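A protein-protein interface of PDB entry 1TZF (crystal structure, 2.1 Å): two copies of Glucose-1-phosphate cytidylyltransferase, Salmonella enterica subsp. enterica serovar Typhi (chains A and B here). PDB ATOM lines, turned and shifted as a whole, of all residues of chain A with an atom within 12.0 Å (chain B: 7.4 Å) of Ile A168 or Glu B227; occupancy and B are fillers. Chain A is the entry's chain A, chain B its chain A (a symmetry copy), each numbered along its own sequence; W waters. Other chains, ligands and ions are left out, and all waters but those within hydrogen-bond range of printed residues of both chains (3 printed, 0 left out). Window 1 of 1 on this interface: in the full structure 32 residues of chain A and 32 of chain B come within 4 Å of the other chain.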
ATOM      1  N   PHE A 163      20.816 -12.794  12.766  1.00  0.00           N
ATOM      2  CA  PHE A 163      19.841 -12.470  11.758  1.00  0.00           C
ATOM      3  C   PHE A 163      20.486 -11.923  10.500  1.00  0.00           C
ATOM      4  O   PHE A 163      21.709 -11.772  10.428  1.00  0.00           O
ATOM      5  CB  PHE A 163      18.810 -11.454  12.327  1.00  0.00           C
ATOM      6  CG  PHE A 163      18.145 -11.978  13.589  1.00  0.00           C
ATOM      7  CD1 PHE A 163      18.627 -11.620  14.852  1.00  0.00           C
ATOM      8  CD2 PHE A 163      17.062 -12.859  13.530  1.00  0.00           C
ATOM      9  CE1 PHE A 163      18.052 -12.123  16.026  1.00  0.00           C
ATOM     10  CE2 PHE A 163      16.475 -13.367  14.694  1.00  0.00           C
ATOM     11  CZ  PHE A 163      16.974 -13.007  15.950  1.00  0.00           C
ATOM     12  N   GLY A 164      19.626 -11.650   9.503  1.00  0.00           N
ATOM     13  CA  GLY A 164      20.046 -11.061   8.237  1.00  0.00           C
ATOM     14  C   GLY A 164      20.267  -9.553   8.476  1.00  0.00           C
ATOM     15  O   GLY A 164      19.325  -8.806   8.789  1.00  0.00           O
ATOM     16  N   ALA A 165      21.518  -9.099   8.380  1.00  0.00           N
ATOM     17  CA  ALA A 165      21.845  -7.676   8.592  1.00  0.00           C
ATOM     18  C   ALA A 165      21.456  -6.771   7.426  1.00  0.00           C
ATOM     19  O   ALA A 165      21.624  -7.147   6.256  1.00  0.00           O
ATOM     20  CB  ALA A 165      23.326  -7.504   8.866  1.00  0.00           C
ATOM     21  N   LEU A 166      20.953  -5.564   7.751  1.00  0.00           N
ATOM     22  CA  LEU A 166      20.513  -4.627   6.712  1.00  0.00           C
ATOM     23  C   LEU A 166      21.145  -3.239   6.683  1.00  0.00           C
ATOM     24  O   LEU A 166      21.335  -2.635   7.735  1.00  0.00           O
ATOM     25  CB  LEU A 166      18.984  -4.409   6.793  1.00  0.00           C
ATOM     26  CG  LEU A 166      18.165  -5.697   6.871  1.00  0.00           C
ATOM     27  CD1 LEU A 166      16.693  -5.372   7.118  1.00  0.00           C
ATOM     28  CD2 LEU A 166      18.322  -6.548   5.600  1.00  0.00           C
ATOM     29  N   ASP A 167      21.405  -2.724   5.462  1.00  0.00           N
ATOM     30  CA  ASP A 167      21.925  -1.353   5.250  1.00  0.00           C
ATOM     31  C   ASP A 167      20.825  -0.590   4.544  1.00  0.00           C
ATOM     32  O   ASP A 167      20.657  -0.639   3.323  1.00  0.00           O
ATOM     33  CB  ASP A 167      23.268  -1.218   4.499  1.00  0.00           C
ATOM     34  CG  ASP A 167      23.820   0.199   4.511  1.00  0.00           C
ATOM     35  OD1 ASP A 167      23.306   1.123   5.119  1.00  0.00           O
ATOM     36  OD2 ASP A 167      24.915   0.330   3.806  1.00  0.00           O
ATOM     37  N   ILE A 168      20.009   0.083   5.342  1.00  0.00           N
ATOM     38  CA  ILE A 168      18.881   0.802   4.783  1.00  0.00           C
ATOM     39  C   ILE A 168      19.018   2.293   4.701  1.00  0.00           C
ATOM     40  O   ILE A 168      19.499   2.983   5.617  1.00  0.00           O
ATOM     41  CB  ILE A 168      17.595   0.539   5.523  1.00  0.00           C
ATOM     42  CG1 ILE A 168      17.279  -0.943   5.548  1.00  0.00           C
ATOM     43  CG2 ILE A 168      16.469   1.318   4.861  1.00  0.00           C
ATOM     44  CD1 ILE A 168      16.753  -1.327   6.927  1.00  0.00           C
ATOM     45  N   GLN A 169      18.521   2.756   3.578  1.00  0.00           N
ATOM     46  CA  GLN A 169      18.522   4.155   3.326  1.00  0.00           C
ATOM     47  C   GLN A 169      17.375   4.551   2.474  1.00  0.00           C
ATOM     48  O   GLN A 169      17.156   4.010   1.381  1.00  0.00           O
ATOM     49  CB  GLN A 169      19.893   4.515   2.727  1.00  0.00           C
ATOM     50  CG  GLN A 169      20.901   4.975   3.822  1.00  0.00           C
ATOM     51  CD  GLN A 169      22.115   4.079   4.099  1.00  0.00           C
ATOM     52  OE1 GLN A 169      22.449   3.161   3.331  1.00  0.00           O
ATOM     53  NE2 GLN A 169      22.812   4.378   5.201  1.00  0.00           N
ATOM     54  N   ALA A 170      16.641   5.503   3.005  1.00  0.00           N
ATOM     55  CA  ALA A 170      15.503   5.952   2.252  1.00  0.00           C
ATOM     56  C   ALA A 170      14.571   4.790   1.877  1.00  0.00           C
ATOM     57  O   ALA A 170      13.995   4.778   0.776  1.00  0.00           O
ATOM     58  CB  ALA A 170      15.950   6.727   1.014  1.00  0.00           C
ATOM     59  N   GLY A 171      14.419   3.825   2.812  1.00  0.00           N
ATOM     60  CA  GLY A 171      13.541   2.666   2.618  1.00  0.00           C
ATOM     61  C   GLY A 171      14.134   1.649   1.671  1.00  0.00           C
ATOM     62  O   GLY A 171      13.558   0.612   1.386  1.00  0.00           O
ATOM     63  N   GLN A 172      15.319   1.938   1.191  1.00  0.00           N
ATOM     64  CA  GLN A 172      15.918   1.023   0.307  1.00  0.00           C
ATOM     65  C   GLN A 172      17.024   0.301   0.999  1.00  0.00           C
ATOM     66  O   GLN A 172      17.839   0.932   1.661  1.00  0.00           O
ATOM     67  CB  GLN A 172      16.510   1.867  -0.809  1.00  0.00           C
ATOM     68  CG  GLN A 172      17.655   1.167  -1.542  1.00  0.00           C
ATOM     69  CD  GLN A 172      17.535   1.436  -3.024  1.00  0.00           C
ATOM     70  OE1 GLN A 172      18.522   1.412  -3.775  1.00  0.00           O
ATOM     71  NE2 GLN A 172      16.307   1.727  -3.445  1.00  0.00           N
ATOM     72  N   VAL A 173      17.036  -1.026   0.825  1.00  0.00           N
ATOM     73  CA  VAL A 173      18.078  -1.867   1.394  1.00  0.00           C
ATOM     74  C   VAL A 173      19.268  -1.785   0.479  1.00  0.00           C
ATOM     75  O   VAL A 173      19.283  -2.364  -0.592  1.00  0.00           O
ATOM     76  CB  VAL A 173      17.696  -3.339   1.524  1.00  0.00           C
ATOM     77  CG1 VAL A 173      18.877  -4.156   2.076  1.00  0.00           C
ATOM     78  CG2 VAL A 173      16.435  -3.460   2.382  1.00  0.00           C
ATOM     79  N   ARG A 174      20.253  -1.038   0.901  1.00  0.00           N
ATOM     80  CA  ARG A 174      21.428  -0.881   0.090  1.00  0.00           C
ATOM     81  C   ARG A 174      22.295  -2.139   0.037  1.00  0.00           C
ATOM     82  O   ARG A 174      22.922  -2.451  -0.978  1.00  0.00           O
ATOM     83  CB  ARG A 174      22.182   0.392   0.489  1.00  0.00           C
ATOM     84  CG  ARG A 174      21.404   1.683   0.155  1.00  0.00           C
ATOM     85  CD  ARG A 174      22.161   2.955   0.553  1.00  0.00           C
ATOM     86  NE  ARG A 174      23.424   3.235  -0.173  1.00  0.00           N
ATOM     87  CZ  ARG A 174      24.646   3.316   0.394  1.00  0.00           C
ATOM     88  NH1 ARG A 174      24.856   3.129   1.689  1.00  0.00           N
ATOM     89  NH2 ARG A 174      25.705   3.590  -0.352  1.00  0.00           N
ATOM     90  N   SER A 175      22.313  -2.874   1.139  1.00  0.00           N
ATOM     91  CA  SER A 175      23.095  -4.080   1.255  1.00  0.00           C
ATOM     92  C   SER A 175      22.460  -5.037   2.253  1.00  0.00           C
ATOM     93  O   SER A 175      21.777  -4.616   3.203  1.00  0.00           O
ATOM     94  CB  SER A 175      24.533  -3.742   1.635  1.00  0.00           C
ATOM     95  OG  SER A 175      24.813  -4.072   2.981  1.00  0.00           O
ATOM     96  N   PHE A 176      22.678  -6.325   1.997  1.00  0.00           N
ATOM     97  CA  PHE A 176      22.161  -7.415   2.810  1.00  0.00           C
ATOM     98  C   PHE A 176      23.268  -8.381   3.147  1.00  0.00           C
ATOM     99  O   PHE A 176      23.984  -8.791   2.245  1.00  0.00           O
ATOM    100  CB  PHE A 176      21.077  -8.239   2.073  1.00  0.00           C
ATOM    101  CG  PHE A 176      20.462  -9.303   2.980  1.00  0.00           C
ATOM    102  CD1 PHE A 176      19.248  -9.072   3.634  1.00  0.00           C
ATOM    103  CD2 PHE A 176      21.093 -10.525   3.218  1.00  0.00           C
ATOM    104  CE1 PHE A 176      18.671 -10.011   4.494  1.00  0.00           C
ATOM    105  CE2 PHE A 176      20.529 -11.477   4.074  1.00  0.00           C
ATOM    106  CZ  PHE A 176      19.311 -11.231   4.711  1.00  0.00           C
ATOM    107  N   GLN A 177      23.395  -8.747   4.423  1.00  0.00           N
ATOM    108  CA  GLN A 177      24.405  -9.697   4.906  1.00  0.00           C
ATOM    109  C   GLN A 177      23.777 -10.643   5.914  1.00  0.00           C
ATOM    110  O   GLN A 177      23.223 -10.235   6.942  1.00  0.00           O
ATOM    111  CB  GLN A 177      25.640  -9.020   5.566  1.00  0.00           C
ATOM    112  CG  GLN A 177      27.011  -9.446   4.997  1.00  0.00           C
ATOM    113  CD  GLN A 177      27.056 -10.877   4.465  1.00  0.00           C
ATOM    114  OE1 GLN A 177      26.864 -11.128   3.270  1.00  0.00           O
ATOM    115  NE2 GLN A 177      27.328 -11.835   5.348  1.00  0.00           N
ATOM    116  N   PRO A 180      26.225 -11.564   9.918  1.00  0.00           N
ATOM    117  CA  PRO A 180      27.557 -10.995   9.902  1.00  0.00           C
ATOM    118  C   PRO A 180      28.165 -10.905  11.308  1.00  0.00           C
ATOM    119  O   PRO A 180      27.477 -10.842  12.322  1.00  0.00           O
ATOM    120  CB  PRO A 180      27.377  -9.589   9.346  1.00  0.00           C
ATOM    121  CG  PRO A 180      25.886  -9.277   9.392  1.00  0.00           C
ATOM    122  CD  PRO A 180      25.153 -10.574   9.652  1.00  0.00           C
ATOM    123  N   LEU B 136       2.165  -7.154  12.248  1.00  0.00           N
ATOM    124  CA  LEU B 136       2.410  -6.477  10.989  1.00  0.00           C
ATOM    125  C   LEU B 136       1.185  -6.290  10.079  1.00  0.00           C
ATOM    126  O   LEU B 136       0.347  -7.184   9.893  1.00  0.00           O
ATOM    127  CB  LEU B 136       3.675  -7.064  10.276  1.00  0.00           C
ATOM    128  CG  LEU B 136       3.908  -6.718   8.783  1.00  0.00           C
ATOM    129  CD1 LEU B 136       4.920  -5.595   8.629  1.00  0.00           C
ATOM    130  CD2 LEU B 136       4.456  -7.920   8.001  1.00  0.00           C
ATOM    131  N   THR B 141       2.148  -3.720   3.653  1.00  0.00           N
ATOM    132  CA  THR B 141       3.366  -4.120   2.990  1.00  0.00           C
ATOM    133  C   THR B 141       3.132  -4.393   1.519  1.00  0.00           C
ATOM    134  O   THR B 141       4.011  -4.166   0.697  1.00  0.00           O
ATOM    135  CB  THR B 141       4.060  -5.323   3.666  1.00  0.00           C
ATOM    136  OG1 THR B 141       3.297  -6.494   3.426  1.00  0.00           O
ATOM    137  CG2 THR B 141       4.237  -5.080   5.159  1.00  0.00           C
ATOM    138  N   PHE B 144       2.641  -1.106  -0.152  1.00  0.00           N
ATOM    139  CA  PHE B 144       3.975  -0.534  -0.202  1.00  0.00           C
ATOM    140  C   PHE B 144       4.801  -1.131  -1.351  1.00  0.00           C
ATOM    141  O   PHE B 144       5.471  -0.414  -2.089  1.00  0.00           O
ATOM    142  CB  PHE B 144       4.696  -0.786   1.135  1.00  0.00           C
ATOM    143  CG  PHE B 144       6.169  -0.386   1.205  1.00  0.00           C
ATOM    144  CD1 PHE B 144       6.556   0.839   1.751  1.00  0.00           C
ATOM    145  CD2 PHE B 144       7.184  -1.240   0.775  1.00  0.00           C
ATOM    146  CE1 PHE B 144       7.899   1.217   1.840  1.00  0.00           C
ATOM    147  CE2 PHE B 144       8.534  -0.888   0.857  1.00  0.00           C
ATOM    148  CZ  PHE B 144       8.894   0.351   1.385  1.00  0.00           C
ATOM    149  N   LEU B 154      11.177  -6.451   1.828  1.00  0.00           N
ATOM    150  CA  LEU B 154      11.312  -7.247   3.046  1.00  0.00           C
ATOM    151  C   LEU B 154      10.799  -6.456   4.246  1.00  0.00           C
ATOM    152  O   LEU B 154      10.705  -5.234   4.191  1.00  0.00           O
ATOM    153  CB  LEU B 154      12.687  -7.867   3.356  1.00  0.00           C
ATOM    154  CG  LEU B 154      13.843  -6.891   3.573  1.00  0.00           C
ATOM    155  CD1 LEU B 154      13.821  -6.261   4.974  1.00  0.00           C
ATOM    156  CD2 LEU B 154      15.137  -7.685   3.407  1.00  0.00           C
ATOM    157  N   THR B 155      10.443  -7.136   5.334  1.00  0.00           N
ATOM    158  CA  THR B 155      10.016  -6.434   6.537  1.00  0.00           C
ATOM    159  C   THR B 155      11.203  -6.359   7.490  1.00  0.00           C
ATOM    160  O   THR B 155      11.759  -7.400   7.918  1.00  0.00           O
ATOM    161  CB  THR B 155       8.808  -7.063   7.242  1.00  0.00           C
ATOM    162  OG1 THR B 155       7.767  -7.168   6.292  1.00  0.00           O
ATOM    163  CG2 THR B 155       8.358  -6.194   8.424  1.00  0.00           C
ATOM    164  N   ALA B 156      11.594  -5.113   7.775  1.00  0.00           N
ATOM    165  CA  ALA B 156      12.698  -4.845   8.686  1.00  0.00           C
ATOM    166  C   ALA B 156      12.162  -4.751  10.113  1.00  0.00           C
ATOM    167  O   ALA B 156      11.112  -4.169  10.369  1.00  0.00           O
ATOM    168  CB  ALA B 156      13.526  -3.643   8.278  1.00  0.00           C
ATOM    169  N   THR B 157      12.859  -5.383  11.046  1.00  0.00           N
ATOM    170  CA  THR B 157      12.389  -5.397  12.417  1.00  0.00           C
ATOM    171  C   THR B 157      13.505  -5.308  13.421  1.00  0.00           C
ATOM    172  O   THR B 157      14.659  -5.511  13.100  1.00  0.00           O
ATOM    173  CB  THR B 157      11.703  -6.749  12.709  1.00  0.00           C
ATOM    174  OG1 THR B 157      12.588  -7.824  12.415  1.00  0.00           O
ATOM    175  CG2 THR B 157      10.393  -6.889  11.949  1.00  0.00           C
ATOM    176  N   PHE B 158      13.113  -5.061  14.664  1.00  0.00           N
ATOM    177  CA  PHE B 158      14.035  -5.029  15.786  1.00  0.00           C
ATOM    178  C   PHE B 158      14.032  -6.425  16.384  1.00  0.00           C
ATOM    179  O   PHE B 158      12.989  -7.022  16.704  1.00  0.00           O
ATOM    180  CB  PHE B 158      13.571  -4.048  16.857  1.00  0.00           C
ATOM    181  CG  PHE B 158      13.723  -2.669  16.330  1.00  0.00           C
ATOM    182  CD1 PHE B 158      12.601  -1.910  16.001  1.00  0.00           C
ATOM    183  CD2 PHE B 158      15.006  -2.156  16.129  1.00  0.00           C
ATOM    184  CE1 PHE B 158      12.766  -0.617  15.503  1.00  0.00           C
ATOM    185  CE2 PHE B 158      15.189  -0.861  15.647  1.00  0.00           C
ATOM    186  CZ  PHE B 158      14.057  -0.108  15.336  1.00  0.00           C
ATOM    187  N   ALA B 185      20.052  -1.357  14.900  1.00  0.00           N
ATOM    188  CA  ALA B 185      19.726  -1.607  13.526  1.00  0.00           C
ATOM    189  C   ALA B 185      18.667  -2.682  13.371  1.00  0.00           C
ATOM    190  O   ALA B 185      18.686  -3.683  14.056  1.00  0.00           O
ATOM    191  CB  ALA B 185      20.990  -1.910  12.732  1.00  0.00           C
ATOM    192  N   MET B 186      17.755  -2.430  12.442  1.00  0.00           N
ATOM    193  CA  MET B 186      16.685  -3.326  12.100  1.00  0.00           C
ATOM    194  C   MET B 186      17.277  -4.493  11.317  1.00  0.00           C
ATOM    195  O   MET B 186      18.321  -4.401  10.670  1.00  0.00           O
ATOM    196  CB  MET B 186      15.650  -2.564  11.259  1.00  0.00           C
ATOM    197  CG  MET B 186      15.013  -1.467  12.105  1.00  0.00           C
ATOM    198  SD  MET B 186      13.578  -0.677  11.328  1.00  0.00           S
ATOM    199  CE  MET B 186      12.206  -1.721  11.871  1.00  0.00           C
ATOM    200  N   ILE B 187      16.625  -5.622  11.377  1.00  0.00           N
ATOM    201  CA  ILE B 187      17.151  -6.750  10.665  1.00  0.00           C
ATOM    202  C   ILE B 187      16.078  -7.316   9.783  1.00  0.00           C
ATOM    203  O   ILE B 187      14.989  -6.740   9.758  1.00  0.00           O
ATOM    204  CB  ILE B 187      17.658  -7.783  11.634  1.00  0.00           C
ATOM    205  CG1 ILE B 187      16.617  -7.975  12.751  1.00  0.00           C
ATOM    206  CG2 ILE B 187      18.973  -7.265  12.181  1.00  0.00           C
ATOM    207  CD1 ILE B 187      15.394  -8.840  12.375  1.00  0.00           C
ATOM    208  N   LEU B 223      15.752  -4.136  -3.871  1.00  0.00           N
ATOM    209  CA  LEU B 223      15.245  -4.523  -2.580  1.00  0.00           C
ATOM    210  C   LEU B 223      14.925  -3.365  -1.618  1.00  0.00           C
ATOM    211  O   LEU B 223      15.790  -2.593  -1.184  1.00  0.00           O
ATOM    212  CB  LEU B 223      16.176  -5.602  -2.000  1.00  0.00           C
ATOM    213  CG  LEU B 223      15.882  -5.993  -0.560  1.00  0.00           C
ATOM    214  CD1 LEU B 223      14.635  -6.883  -0.474  1.00  0.00           C
ATOM    215  CD2 LEU B 223      17.112  -6.729  -0.034  1.00  0.00           C
ATOM    216  N   MET B 224      13.632  -3.279  -1.295  1.00  0.00           N
ATOM    217  CA  MET B 224      13.086  -2.294  -0.386  1.00  0.00           C
ATOM    218  C   MET B 224      12.808  -2.865   0.996  1.00  0.00           C
ATOM    219  O   MET B 224      12.599  -4.075   1.180  1.00  0.00           O
ATOM    220  CB  MET B 224      11.808  -1.632  -0.961  1.00  0.00           C
ATOM    221  CG  MET B 224      12.023  -1.068  -2.364  1.00  0.00           C
ATOM    222  SD  MET B 224      13.156   0.351  -2.403  1.00  0.00           S
ATOM    223  CE  MET B 224      12.176   1.548  -1.463  1.00  0.00           C
ATOM    224  N   ALA B 225      12.781  -1.965   1.979  1.00  0.00           N
ATOM    225  CA  ALA B 225      12.511  -2.331   3.362  1.00  0.00           C
ATOM    226  C   ALA B 225      11.294  -1.636   3.945  1.00  0.00           C
ATOM    227  O   ALA B 225      11.207  -0.419   3.971  1.00  0.00           O
ATOM    228  CB  ALA B 225      13.710  -2.030   4.244  1.00  0.00           C
ATOM    229  N   PHE B 226      10.340  -2.421   4.417  1.00  0.00           N
ATOM    230  CA  PHE B 226       9.158  -1.888   5.051  1.00  0.00           C
ATOM    231  C   PHE B 226       9.498  -1.980   6.518  1.00  0.00           C
ATOM    232  O   PHE B 226       9.619  -3.079   7.060  1.00  0.00           O
ATOM    233  CB  PHE B 226       7.964  -2.783   4.749  1.00  0.00           C
ATOM    234  CG  PHE B 226       6.683  -2.325   5.399  1.00  0.00           C
ATOM    235  CD1 PHE B 226       5.731  -1.658   4.625  1.00  0.00           C
ATOM    236  CD2 PHE B 226       6.412  -2.571   6.749  1.00  0.00           C
ATOM    237  CE1 PHE B 226       4.522  -1.233   5.177  1.00  0.00           C
ATOM    238  CE2 PHE B 226       5.204  -2.163   7.316  1.00  0.00           C
ATOM    239  CZ  PHE B 226       4.266  -1.492   6.526  1.00  0.00           C
ATOM    240  N   GLU B 227       9.718  -0.848   7.145  1.00  0.00           N
ATOM    241  CA  GLU B 227      10.107  -0.897   8.529  1.00  0.00           C
ATOM    242  C   GLU B 227       8.959  -1.050   9.479  1.00  0.00           C
ATOM    243  O   GLU B 227       7.983  -0.289   9.424  1.00  0.00           O
ATOM    244  CB  GLU B 227      10.931   0.311   8.940  1.00  0.00           C
ATOM    245  CG  GLU B 227      12.178   0.506   8.080  1.00  0.00           C
ATOM    246  CD  GLU B 227      12.615   1.939   8.118  1.00  0.00           C
ATOM    247  OE1 GLU B 227      12.166   2.755   8.905  1.00  0.00           O
ATOM    248  OE2 GLU B 227      13.496   2.221   7.200  1.00  0.00           O
ATOM    249  N   HIS B 228       9.118  -2.049  10.353  1.00  0.00           N
ATOM    250  CA  HIS B 228       8.108  -2.359  11.359  1.00  0.00           C
ATOM    251  C   HIS B 228       8.736  -2.201  12.727  1.00  0.00           C
ATOM    252  O   HIS B 228       9.325  -3.175  13.211  1.00  0.00           O
ATOM    253  CB  HIS B 228       7.555  -3.794  11.166  1.00  0.00           C
ATOM    254  CG  HIS B 228       6.514  -4.241  12.165  1.00  0.00           C
ATOM    255  ND1 HIS B 228       5.258  -3.660  12.224  1.00  0.00           N
ATOM    256  CD2 HIS B 228       6.541  -5.244  13.108  1.00  0.00           C
ATOM    257  CE1 HIS B 228       4.560  -4.292  13.191  1.00  0.00           C
ATOM    258  NE2 HIS B 228       5.301  -5.245  13.742  1.00  0.00           N
ATOM    259  N   PRO B 229       8.623  -0.972  13.313  1.00  0.00           N
ATOM    260  CA  PRO B 229       9.210  -0.672  14.614  1.00  0.00           C
ATOM    261  C   PRO B 229       8.496  -1.368  15.761  1.00  0.00           C
ATOM    262  O   PRO B 229       9.031  -1.408  16.870  1.00  0.00           O
ATOM    263  CB  PRO B 229       9.078   0.836  14.788  1.00  0.00           C
ATOM    264  CG  PRO B 229       7.848   1.209  13.989  1.00  0.00           C
ATOM    265  CD  PRO B 229       7.726   0.150  12.909  1.00  0.00           C
ATOM    266  N   GLY B 230       7.293  -1.917  15.489  1.00  0.00           N
ATOM    267  CA  GLY B 230       6.469  -2.613  16.482  1.00  0.00           C
ATOM    268  C   GLY B 230       6.829  -4.079  16.815  1.00  0.00           C
ATOM    269  O   GLY B 230       7.973  -4.512  16.664  1.00  0.00           O
HETATM  270  O   HOH W   1      21.068  -4.979  10.339  1.00  0.00           O
HETATM  271  O   HOH W   2      19.378  -1.431   9.554  1.00  0.00           O
HETATM  272  O   HOH W   3      18.061  -2.514  -2.969  1.00  0.00           O
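N of Ala B225 lies within hydrogen-bond range of O of Gly A171, 2.8 Å away.
The side-chain amide nitrogen (NE2) of Gln A172 is in hydrogen-bond range of the side-chain sulfur (SD) of Met B224 (3.6 Å).
The backbone NH of Val A173 is in hydrogen-bond range of the backbone carbonyl oxygen of Leu B223, at 2.8 Å.
N of Leu B154 sits at hydrogen-bond distance from O of Met B224 (2.8 Å).
The backbone NH (N) of Phe B226 sits at hydrogen-bond distance from the backbone carbonyl oxygen (O) of Leu B154, at 2.8 Å.
The backbone NH (N) of Ala B156 is in hydrogen-bond range of the backbone carbonyl oxygen (O) of Phe B226, 2.9 Å away.
N of His B228 sits at hydrogen-bond distance from O of Ala B156, 2.9 Å away.
O of Thr B157 lies within hydrogen-bond range of N of Ile B187 (2.6 Å).
Phe A163 touches Ile B187 (CB to CB, 3.9 Å).
Gly A164 touches Ile B187 (O to CB, 3.5 Å).
CD1 of Leu A166 touches CD1 of Leu B154, at 3.7 Å.
Leu A166 touches Ala B156.
O of Met B186 touches CB of Leu A166, at 3.9 Å.
C of Ile B187 touches CD1 of Leu A166, 3.4 Å away.
Ala B225 touches Ile A168 (CB to CG1, 3.95 Å).
O of Gly A171 touches CE of Met B224, 3.3 Å away.
Val A173 touches Met B224.
Val A173 touches Ala B225 (CG2 to CB, 3.6 Å).
Printed residues of chain B within 4 Å of Ile A168: Ala B225 and Glu B227.
Glu B227 touches one residue of chain A.
No residue of chain A comes within 4 Å of Thr B155.
Of chain A, only Leu A166 (3.8 Å) comes within 4 Å of Ala B156.
No residue of chain A comes within 4 Å of Pro B229.
Of the printed residues of chain A, Leu B223 touches Gln A172 and Val A173.
Of the printed residues of chain B, Phe A163 touches Ile B187 (3.9 Å).
Printed residues of chain B within 4 Å of Leu A166: Leu B154 (3.7 Å), Ala B156 (3.8 Å), Met B186 (3.9 Å) and Ile B187 (3.4 Å).
Printed residues of chain A within 4 Å of Met B224: Gly A171, Gln A172 and Val A173.
The nearest residue of chain A that does not touch Glu B227 is Gly A171 (4.6 Å).
The nearest printed residue of chain B that does not touch Gln A172 is Ala B225 (4.6 Å).
Of the 19 printed residues of chain B, 8 touch a printed residue of chain A.
Of the 16 printed residues of chain A, 7 touch a printed residue of chain B.
Printed residues of chain A that touch a printed residue of chain B: Phe A163, Gly A164, Leu A166, Ile A168, Gly A171, Gln A172 and Val A173.
Among the printed residues, no Asp or Glu carboxylate lies within 4 Å of a Lys or Arg side-chain nitrogen of the other chain.
No position is printed for both chains.
Of the 15 pairs that touch across the chains among the printed residues, none has its exchanged pair printed and touching as well.
Water W1 lies within hydrogen-bond range of the backbone NH (N) of Leu A166 (2.7 Å) and the backbone carbonyl oxygen (O) of Met B186 (2.8 Å).
Water W3 lies within hydrogen-bond range of O of Val A173 and O of Leu B223.
Water W2 bridges the backbone carbonyl oxygen of Leu A166 (2.9 Å) and the backbone carbonyl oxygen of Met B186 (3.3 Å).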
